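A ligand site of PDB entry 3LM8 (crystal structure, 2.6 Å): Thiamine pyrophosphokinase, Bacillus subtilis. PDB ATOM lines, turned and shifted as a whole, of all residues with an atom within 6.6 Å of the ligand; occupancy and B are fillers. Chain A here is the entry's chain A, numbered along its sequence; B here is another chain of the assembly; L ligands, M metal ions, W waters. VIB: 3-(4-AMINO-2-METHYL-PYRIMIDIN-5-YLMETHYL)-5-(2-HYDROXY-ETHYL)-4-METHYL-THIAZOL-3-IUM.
N of Tyr 174 of chain B sits close to ND2 of Asn 191 of chain B (3.0 Å).
OD2 of Asp 78 lies close to O of Glu 76, at 2.6 Å.
The side-chain hydroxyl (OG1) of Thr 186 of chain B lies within hydrogen-bond range of the side-chain hydroxyl (OG1) of Thr 80 (3.4 Å).
O of Ile 155 of chain B sits at hydrogen-bond distance from N of Asn 191 of chain B.
O of Leu 187 of chain B sits close to N3A of the ligand (3.2 Å).
The backbone carbonyl oxygen (O) of Ile 189 of chain B lies close to a nitrogen (N3) of the ligand (3.3 Å).
Tyr 174 of chain B touches the ligand (CD1 to N4A, 3.3 Å).
Leu 176 of chain B touches the ligand.
Thr 186 of chain B touches the ligand.
CA of Cys 188 of chain B touches N1A of the ligand, at 3.4 Å.
Asn 191 of chain B touches the ligand (CB to C6A, 3.8 Å).
Hydrophobic or aromatic side chains that line the ligand: Tyr 174 of chain B, Leu 176 of chain B and Leu 187 of chain B.
Of the 23 residues printed, 10 come within 4 Å of the ligand.
The nearest printed residue that does not touch the ligand is Thr 80 (4.1 Å).
The side-chain carboxylate (OD1) of Asp 78 sits at hydrogen-bond distance from a nitrogen (N4A) of the ligand, at 3.2 Å.
N4A of the ligand is in hydrogen-bond range of O of Lys 77, 2.7 Å away.
OG of Ser 190 of chain B lies within hydrogen-bond range of O1 of the ligand.
Water W1 bridges the guanidinium group of Arg 106 and an oxygen (O1) of the ligand.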
ATOM      1  N   ALA A  75       1.827 -25.289  16.057  1.00  0.00           N
ATOM      2  CA  ALA A  75       2.570 -24.129  16.534  1.00  0.00           C
ATOM      3  C   ALA A  75       2.171 -22.872  15.758  1.00  0.00           C
ATOM      4  O   ALA A  75       1.376 -22.949  14.816  1.00  0.00           O
ATOM      5  CB  ALA A  75       4.065 -24.374  16.386  1.00  0.00           C
ATOM      6  N   GLU A  76       2.736 -21.728  16.146  1.00  0.00           N
ATOM      7  CA  GLU A  76       2.434 -20.451  15.485  1.00  0.00           C
ATOM      8  C   GLU A  76       3.657 -19.837  14.783  1.00  0.00           C
ATOM      9  O   GLU A  76       3.729 -18.612  14.640  1.00  0.00           O
ATOM     10  CB  GLU A  76       1.889 -19.434  16.497  1.00  0.00           C
ATOM     11  CG  GLU A  76       1.176 -20.029  17.704  1.00  0.00           C
ATOM     12  CD  GLU A  76       0.061 -20.980  17.317  1.00  0.00           C
ATOM     13  OE1 GLU A  76      -0.903 -20.525  16.657  1.00  0.00           O
ATOM     14  OE2 GLU A  76       0.142 -22.171  17.670  1.00  0.00           O
ATOM     15  N   LYS A  77       4.597 -20.679  14.357  1.00  0.00           N
ATOM     16  CA  LYS A  77       5.819 -20.245  13.659  1.00  0.00           C
ATOM     17  C   LYS A  77       6.649 -19.232  14.436  1.00  0.00           C
ATOM     18  O   LYS A  77       7.771 -18.903  14.020  1.00  0.00           O
ATOM     19  CB  LYS A  77       5.477 -19.631  12.292  1.00  0.00           C
ATOM     20  CG  LYS A  77       5.340 -18.100  12.320  1.00  0.00           C
ATOM     21  CD  LYS A  77       4.999 -17.486  10.963  1.00  0.00           C
ATOM     22  CE  LYS A  77       4.785 -15.984  11.096  1.00  0.00           C
ATOM     23  NZ  LYS A  77       4.269 -15.344   9.852  1.00  0.00           N
ATOM     24  N   ASP A  78       6.108 -18.730  15.540  1.00  0.00           N
ATOM     25  CA  ASP A  78       6.805 -17.740  16.359  1.00  0.00           C
ATOM     26  C   ASP A  78       7.228 -18.377  17.669  1.00  0.00           C
ATOM     27  O   ASP A  78       7.930 -17.769  18.495  1.00  0.00           O
ATOM     28  CB  ASP A  78       5.874 -16.561  16.607  1.00  0.00           C
ATOM     29  CG  ASP A  78       5.326 -15.978  15.319  1.00  0.00           C
ATOM     30  OD1 ASP A  78       6.127 -15.463  14.504  1.00  0.00           O
ATOM     31  OD2 ASP A  78       4.088 -16.036  15.118  1.00  0.00           O
ATOM     32  N   GLN A  79       6.802 -19.612  17.846  1.00  0.00           N
ATOM     33  CA  GLN A  79       7.101 -20.406  19.014  1.00  0.00           C
ATOM     34  C   GLN A  79       7.484 -21.761  18.453  1.00  0.00           C
ATOM     35  O   GLN A  79       6.845 -22.238  17.515  1.00  0.00           O
ATOM     36  CB  GLN A  79       5.851 -20.515  19.892  1.00  0.00           C
ATOM     37  CG  GLN A  79       5.866 -21.666  20.874  1.00  0.00           C
ATOM     38  CD  GLN A  79       4.631 -21.675  21.767  1.00  0.00           C
ATOM     39  OE1 GLN A  79       3.501 -21.659  21.283  1.00  0.00           O
ATOM     40  NE2 GLN A  79       4.851 -21.709  23.078  1.00  0.00           N
ATOM     41  N   THR A  80       8.525 -22.366  18.992  1.00  0.00           N
ATOM     42  CA  THR A  80       8.947 -23.676  18.515  1.00  0.00           C
ATOM     43  C   THR A  80       7.928 -24.725  18.971  1.00  0.00           C
ATOM     44  O   THR A  80       7.168 -24.495  19.915  1.00  0.00           O
ATOM     45  CB  THR A  80      10.332 -24.062  19.068  1.00  0.00           C
ATOM     46  OG1 THR A  80      11.294 -23.072  18.678  1.00  0.00           O
ATOM     47  CG2 THR A  80      10.765 -25.410  18.520  1.00  0.00           C
ATOM     48  N   ASP A  81       7.899 -25.860  18.278  1.00  0.00           N
ATOM     49  CA  ASP A  81       6.975 -26.930  18.627  1.00  0.00           C
ATOM     50  C   ASP A  81       7.284 -27.364  20.059  1.00  0.00           C
ATOM     51  O   ASP A  81       6.397 -27.473  20.905  1.00  0.00           O
ATOM     52  CB  ASP A  81       7.165 -28.119  17.683  1.00  0.00           C
ATOM     53  CG  ASP A  81       7.044 -27.725  16.229  1.00  0.00           C
ATOM     54  OD1 ASP A  81       6.103 -26.974  15.890  1.00  0.00           O
ATOM     55  OD2 ASP A  81       7.876 -28.175  15.411  1.00  0.00           O
ATOM     56  N   ARG A 106      22.151 -29.597  13.834  1.00  0.00           N
ATOM     57  CA  ARG A 106      22.047 -28.150  13.900  1.00  0.00           C
ATOM     58  C   ARG A 106      22.233 -27.673  15.318  1.00  0.00           C
ATOM     59  O   ARG A 106      21.441 -28.000  16.190  1.00  0.00           O
ATOM     60  CB  ARG A 106      20.686 -27.696  13.350  1.00  0.00           C
ATOM     61  CG  ARG A 106      20.647 -27.655  11.827  1.00  0.00           C
ATOM     62  CD  ARG A 106      19.849 -26.485  11.330  1.00  0.00           C
ATOM     63  NE  ARG A 106      18.426 -26.724  11.434  1.00  0.00           N
ATOM     64  CZ  ARG A 106      17.499 -25.769  11.504  1.00  0.00           C
ATOM     65  NH1 ARG A 106      17.840 -24.485  11.475  1.00  0.00           N
ATOM     66  NH2 ARG A 106      16.229 -26.117  11.602  1.00  0.00           N
ATOM     67  N   TYR B 154      19.696 -21.845   6.878  1.00  0.00           N
ATOM     68  CA  TYR B 154      19.210 -21.323   8.156  1.00  0.00           C
ATOM     69  C   TYR B 154      20.074 -20.290   8.874  1.00  0.00           C
ATOM     70  O   TYR B 154      21.286 -20.257   8.723  1.00  0.00           O
ATOM     71  CB  TYR B 154      18.904 -22.494   9.102  1.00  0.00           C
ATOM     72  CG  TYR B 154      17.886 -23.464   8.548  1.00  0.00           C
ATOM     73  CD1 TYR B 154      18.266 -24.465   7.640  1.00  0.00           C
ATOM     74  CD2 TYR B 154      16.532 -23.365   8.888  1.00  0.00           C
ATOM     75  CE1 TYR B 154      17.325 -25.339   7.073  1.00  0.00           C
ATOM     76  CE2 TYR B 154      15.582 -24.229   8.322  1.00  0.00           C
ATOM     77  CZ  TYR B 154      15.993 -25.212   7.425  1.00  0.00           C
ATOM     78  OH  TYR B 154      15.054 -26.046   6.860  1.00  0.00           O
ATOM     79  N   ILE B 155      19.408 -19.448   9.664  1.00  0.00           N
ATOM     80  CA  ILE B 155      20.089 -18.415  10.434  1.00  0.00           C
ATOM     81  C   ILE B 155      19.287 -18.115  11.719  1.00  0.00           C
ATOM     82  O   ILE B 155      18.202 -17.537  11.668  1.00  0.00           O
ATOM     83  CB  ILE B 155      20.258 -17.120   9.596  1.00  0.00           C
ATOM     84  CG1 ILE B 155      21.118 -17.416   8.354  1.00  0.00           C
ATOM     85  CG2 ILE B 155      20.890 -16.008  10.446  1.00  0.00           C
ATOM     86  CD1 ILE B 155      21.172 -16.307   7.334  1.00  0.00           C
ATOM     87  N   LEU B 167      16.313  -5.295  18.321  1.00  0.00           N
ATOM     88  CA  LEU B 167      16.860  -6.140  17.275  1.00  0.00           C
ATOM     89  C   LEU B 167      16.104  -5.836  15.998  1.00  0.00           C
ATOM     90  O   LEU B 167      14.878  -5.901  15.967  1.00  0.00           O
ATOM     91  CB  LEU B 167      16.723  -7.637  17.576  1.00  0.00           C
ATOM     92  CG  LEU B 167      17.104  -8.527  16.371  1.00  0.00           C
ATOM     93  CD1 LEU B 167      18.475  -8.138  15.849  1.00  0.00           C
ATOM     94  CD2 LEU B 167      17.096 -10.004  16.739  1.00  0.00           C
ATOM     95  N   LEU B 169      16.022  -6.579  11.700  1.00  0.00           N
ATOM     96  CA  LEU B 169      16.504  -7.481  10.669  1.00  0.00           C
ATOM     97  C   LEU B 169      16.065  -6.972   9.324  1.00  0.00           C
ATOM     98  O   LEU B 169      15.016  -6.353   9.196  1.00  0.00           O
ATOM     99  CB  LEU B 169      15.975  -8.892  10.905  1.00  0.00           C
ATOM    100  CG  LEU B 169      16.349  -9.458  12.265  1.00  0.00           C
ATOM    101  CD1 LEU B 169      15.547 -10.703  12.554  1.00  0.00           C
ATOM    102  CD2 LEU B 169      17.844  -9.769  12.285  1.00  0.00           C
ATOM    103  N   TYR B 174      11.705 -13.708   8.018  1.00  0.00           N
ATOM    104  CA  TYR B 174      10.951 -13.337   9.218  1.00  0.00           C
ATOM    105  C   TYR B 174      11.434 -11.982   9.719  1.00  0.00           C
ATOM    106  O   TYR B 174      12.157 -11.892  10.698  1.00  0.00           O
ATOM    107  CB  TYR B 174      11.136 -14.412  10.311  1.00  0.00           C
ATOM    108  CG  TYR B 174      10.519 -15.734   9.934  1.00  0.00           C
ATOM    109  CD1 TYR B 174       9.152 -15.980  10.121  1.00  0.00           C
ATOM    110  CD2 TYR B 174      11.278 -16.729   9.324  1.00  0.00           C
ATOM    111  CE1 TYR B 174       8.574 -17.183   9.711  1.00  0.00           C
ATOM    112  CE2 TYR B 174      10.711 -17.923   8.914  1.00  0.00           C
ATOM    113  CZ  TYR B 174       9.355 -18.139   9.103  1.00  0.00           C
ATOM    114  OH  TYR B 174       8.798 -19.332   8.684  1.00  0.00           O
ATOM    115  N   PRO B 175      11.020 -10.898   9.047  1.00  0.00           N
ATOM    116  CA  PRO B 175      11.372  -9.508   9.363  1.00  0.00           C
ATOM    117  C   PRO B 175      11.228  -9.154  10.831  1.00  0.00           C
ATOM    118  O   PRO B 175      10.352  -9.679  11.522  1.00  0.00           O
ATOM    119  CB  PRO B 175      10.407  -8.715   8.504  1.00  0.00           C
ATOM    120  CG  PRO B 175      10.269  -9.563   7.295  1.00  0.00           C
ATOM    121  CD  PRO B 175      10.096 -10.939   7.900  1.00  0.00           C
ATOM    122  N   LEU B 176      12.074  -8.261  11.303  1.00  0.00           N
ATOM    123  CA  LEU B 176      12.038  -7.831  12.699  1.00  0.00           C
ATOM    124  C   LEU B 176      12.438  -6.344  12.771  1.00  0.00           C
ATOM    125  O   LEU B 176      13.461  -5.943  12.202  1.00  0.00           O
ATOM    126  CB  LEU B 176      12.990  -8.701  13.515  1.00  0.00           C
ATOM    127  CG  LEU B 176      12.631  -9.075  14.947  1.00  0.00           C
ATOM    128  CD1 LEU B 176      11.237  -9.684  14.990  1.00  0.00           C
ATOM    129  CD2 LEU B 176      13.670 -10.060  15.463  1.00  0.00           C
ATOM    130  N   ILE B 181      14.013  -8.814  22.215  1.00  0.00           N
ATOM    131  CA  ILE B 181      14.075 -10.259  22.417  1.00  0.00           C
ATOM    132  C   ILE B 181      14.510 -10.630  23.837  1.00  0.00           C
ATOM    133  O   ILE B 181      15.640 -10.383  24.240  1.00  0.00           O
ATOM    134  CB  ILE B 181      15.082 -10.923  21.420  1.00  0.00           C
ATOM    135  CG1 ILE B 181      14.910 -10.358  20.009  1.00  0.00           C
ATOM    136  CG2 ILE B 181      14.860 -12.432  21.386  1.00  0.00           C
ATOM    137  CD1 ILE B 181      13.603 -10.726  19.363  1.00  0.00           C
ATOM    138  N   THR B 186      12.825 -18.194  21.898  1.00  0.00           N
ATOM    139  CA  THR B 186      13.225 -19.028  20.775  1.00  0.00           C
ATOM    140  C   THR B 186      12.587 -18.401  19.545  1.00  0.00           C
ATOM    141  O   THR B 186      12.621 -18.973  18.455  1.00  0.00           O
ATOM    142  CB  THR B 186      12.726 -20.478  20.941  1.00  0.00           C
ATOM    143  OG1 THR B 186      11.290 -20.492  20.962  1.00  0.00           O
ATOM    144  CG2 THR B 186      13.253 -21.070  22.227  1.00  0.00           C
ATOM    145  N   LEU B 187      12.000 -17.229  19.719  1.00  0.00           N
ATOM    146  CA  LEU B 187      11.350 -16.556  18.610  1.00  0.00           C
ATOM    147  C   LEU B 187      12.215 -16.451  17.362  1.00  0.00           C
ATOM    148  O   LEU B 187      11.720 -16.669  16.259  1.00  0.00           O
ATOM    149  CB  LEU B 187      10.908 -15.141  18.999  1.00  0.00           C
ATOM    150  CG  LEU B 187      10.494 -14.288  17.788  1.00  0.00           C
ATOM    151  CD1 LEU B 187       9.334 -14.951  17.038  1.00  0.00           C
ATOM    152  CD2 LEU B 187      10.099 -12.907  18.218  1.00  0.00           C
ATOM    153  N   CYS B 188      13.492 -16.113  17.535  1.00  0.00           N
ATOM    154  CA  CYS B 188      14.398 -15.914  16.403  1.00  0.00           C
ATOM    155  C   CYS B 188      15.198 -17.116  15.907  1.00  0.00           C
ATOM    156  O   CYS B 188      16.174 -16.947  15.188  1.00  0.00           O
ATOM    157  CB  CYS B 188      15.375 -14.792  16.729  1.00  0.00           C
ATOM    158  SG  CYS B 188      14.592 -13.291  17.256  1.00  0.00           S
ATOM    159  N   ILE B 189      14.796 -18.310  16.297  1.00  0.00           N
ATOM    160  CA  ILE B 189      15.517 -19.478  15.819  1.00  0.00           C
ATOM    161  C   ILE B 189      15.089 -19.829  14.394  1.00  0.00           C
ATOM    162  O   ILE B 189      13.920 -19.675  14.044  1.00  0.00           O
ATOM    163  CB  ILE B 189      15.320 -20.685  16.749  1.00  0.00           C
ATOM    164  CG1 ILE B 189      16.178 -20.494  18.009  1.00  0.00           C
ATOM    165  CG2 ILE B 189      15.684 -21.972  16.030  1.00  0.00           C
ATOM    166  CD1 ILE B 189      16.014 -21.547  19.066  1.00  0.00           C
ATOM    167  N   SER B 190      16.049 -20.288  13.602  1.00  0.00           N
ATOM    168  CA  SER B 190      15.897 -20.686  12.198  1.00  0.00           C
ATOM    169  C   SER B 190      15.135 -19.733  11.284  1.00  0.00           C
ATOM    170  O   SER B 190      14.067 -20.049  10.732  1.00  0.00           O
ATOM    171  CB  SER B 190      15.333 -22.111  12.071  1.00  0.00           C
ATOM    172  OG  SER B 190      14.040 -22.204  12.598  1.00  0.00           O
ATOM    173  N   ASN B 191      15.706 -18.558  11.122  1.00  0.00           N
ATOM    174  CA  ASN B 191      15.156 -17.550  10.250  1.00  0.00           C
ATOM    175  C   ASN B 191      15.918 -17.857   8.963  1.00  0.00           C
ATOM    176  O   ASN B 191      16.809 -18.693   8.956  1.00  0.00           O
ATOM    177  CB  ASN B 191      15.529 -16.159  10.788  1.00  0.00           C
ATOM    178  CG  ASN B 191      14.724 -15.054  10.158  1.00  0.00           C
ATOM    179  OD1 ASN B 191      14.765 -13.900  10.601  1.00  0.00           O
ATOM    180  ND2 ASN B 191      13.968 -15.390   9.118  1.00  0.00           N
ATOM    181  N   GLU B 192      15.535 -17.221   7.866  1.00  0.00           N
ATOM    182  CA  GLU B 192      16.203 -17.423   6.588  1.00  0.00           C
ATOM    183  C   GLU B 192      16.505 -16.074   5.969  1.00  0.00           C
ATOM    184  O   GLU B 192      16.025 -15.051   6.443  1.00  0.00           O
ATOM    185  CB  GLU B 192      15.341 -18.257   5.646  1.00  0.00           C
ATOM    186  CG  GLU B 192      15.120 -19.686   6.126  1.00  0.00           C
ATOM    187  CD  GLU B 192      14.240 -20.499   5.184  1.00  0.00           C
ATOM    188  OE1 GLU B 192      14.552 -20.552   3.975  1.00  0.00           O
ATOM    189  OE2 GLU B 192      13.239 -21.089   5.667  1.00  0.00           O
HETATM  190  CM2 VIB L   1      11.941 -13.077  14.513  1.00  0.00           C
HETATM  191  N4A VIB L   1       8.889 -16.587  13.313  1.00  0.00           N
HETATM  192  CM4 VIB L   1      10.019 -20.980  11.579  1.00  0.00           C
HETATM  193  O1  VIB L   1      12.055 -23.593  13.777  1.00  0.00           O
HETATM  194  C7  VIB L   1      10.933 -23.739  14.650  1.00  0.00           C
HETATM  195  C6  VIB L   1       9.766 -22.887  14.134  1.00  0.00           C
HETATM  196  C2  VIB L   1      10.925 -19.045  14.605  1.00  0.00           C
HETATM  197  S1  VIB L   1      10.347 -20.418  15.521  1.00  0.00           S
HETATM  198  C5  VIB L   1      10.130 -21.403  14.093  1.00  0.00           C
HETATM  199  C4  VIB L   1      10.312 -20.551  13.010  1.00  0.00           C
HETATM  200  N3  VIB L   1      10.746 -19.326  13.314  1.00  0.00           N
HETATM  201  C7A VIB L   1      10.986 -18.318  12.269  1.00  0.00           C
HETATM  202  C4A VIB L   1      10.138 -16.143  13.378  1.00  0.00           C
HETATM  203  N3A VIB L   1      10.401 -14.925  13.884  1.00  0.00           N
HETATM  204  C2A VIB L   1      11.660 -14.472  13.950  1.00  0.00           C
HETATM  205  N1A VIB L   1      12.676 -15.229  13.510  1.00  0.00           N
HETATM  206  C6A VIB L   1      12.464 -16.429  12.997  1.00  0.00           C
HETATM  207  C5A VIB L   1      11.183 -16.940  12.908  1.00  0.00           C
HETATM  208 MG    MG M   1       8.272 -26.351  11.377  1.00  0.00          MG
HETATM  209  O   HOH W   1      13.694 -25.538  11.462  1.00  0.00           O
HETATM  210  O   HOH W   2      15.434 -14.526  13.586  1.00  0.00           O
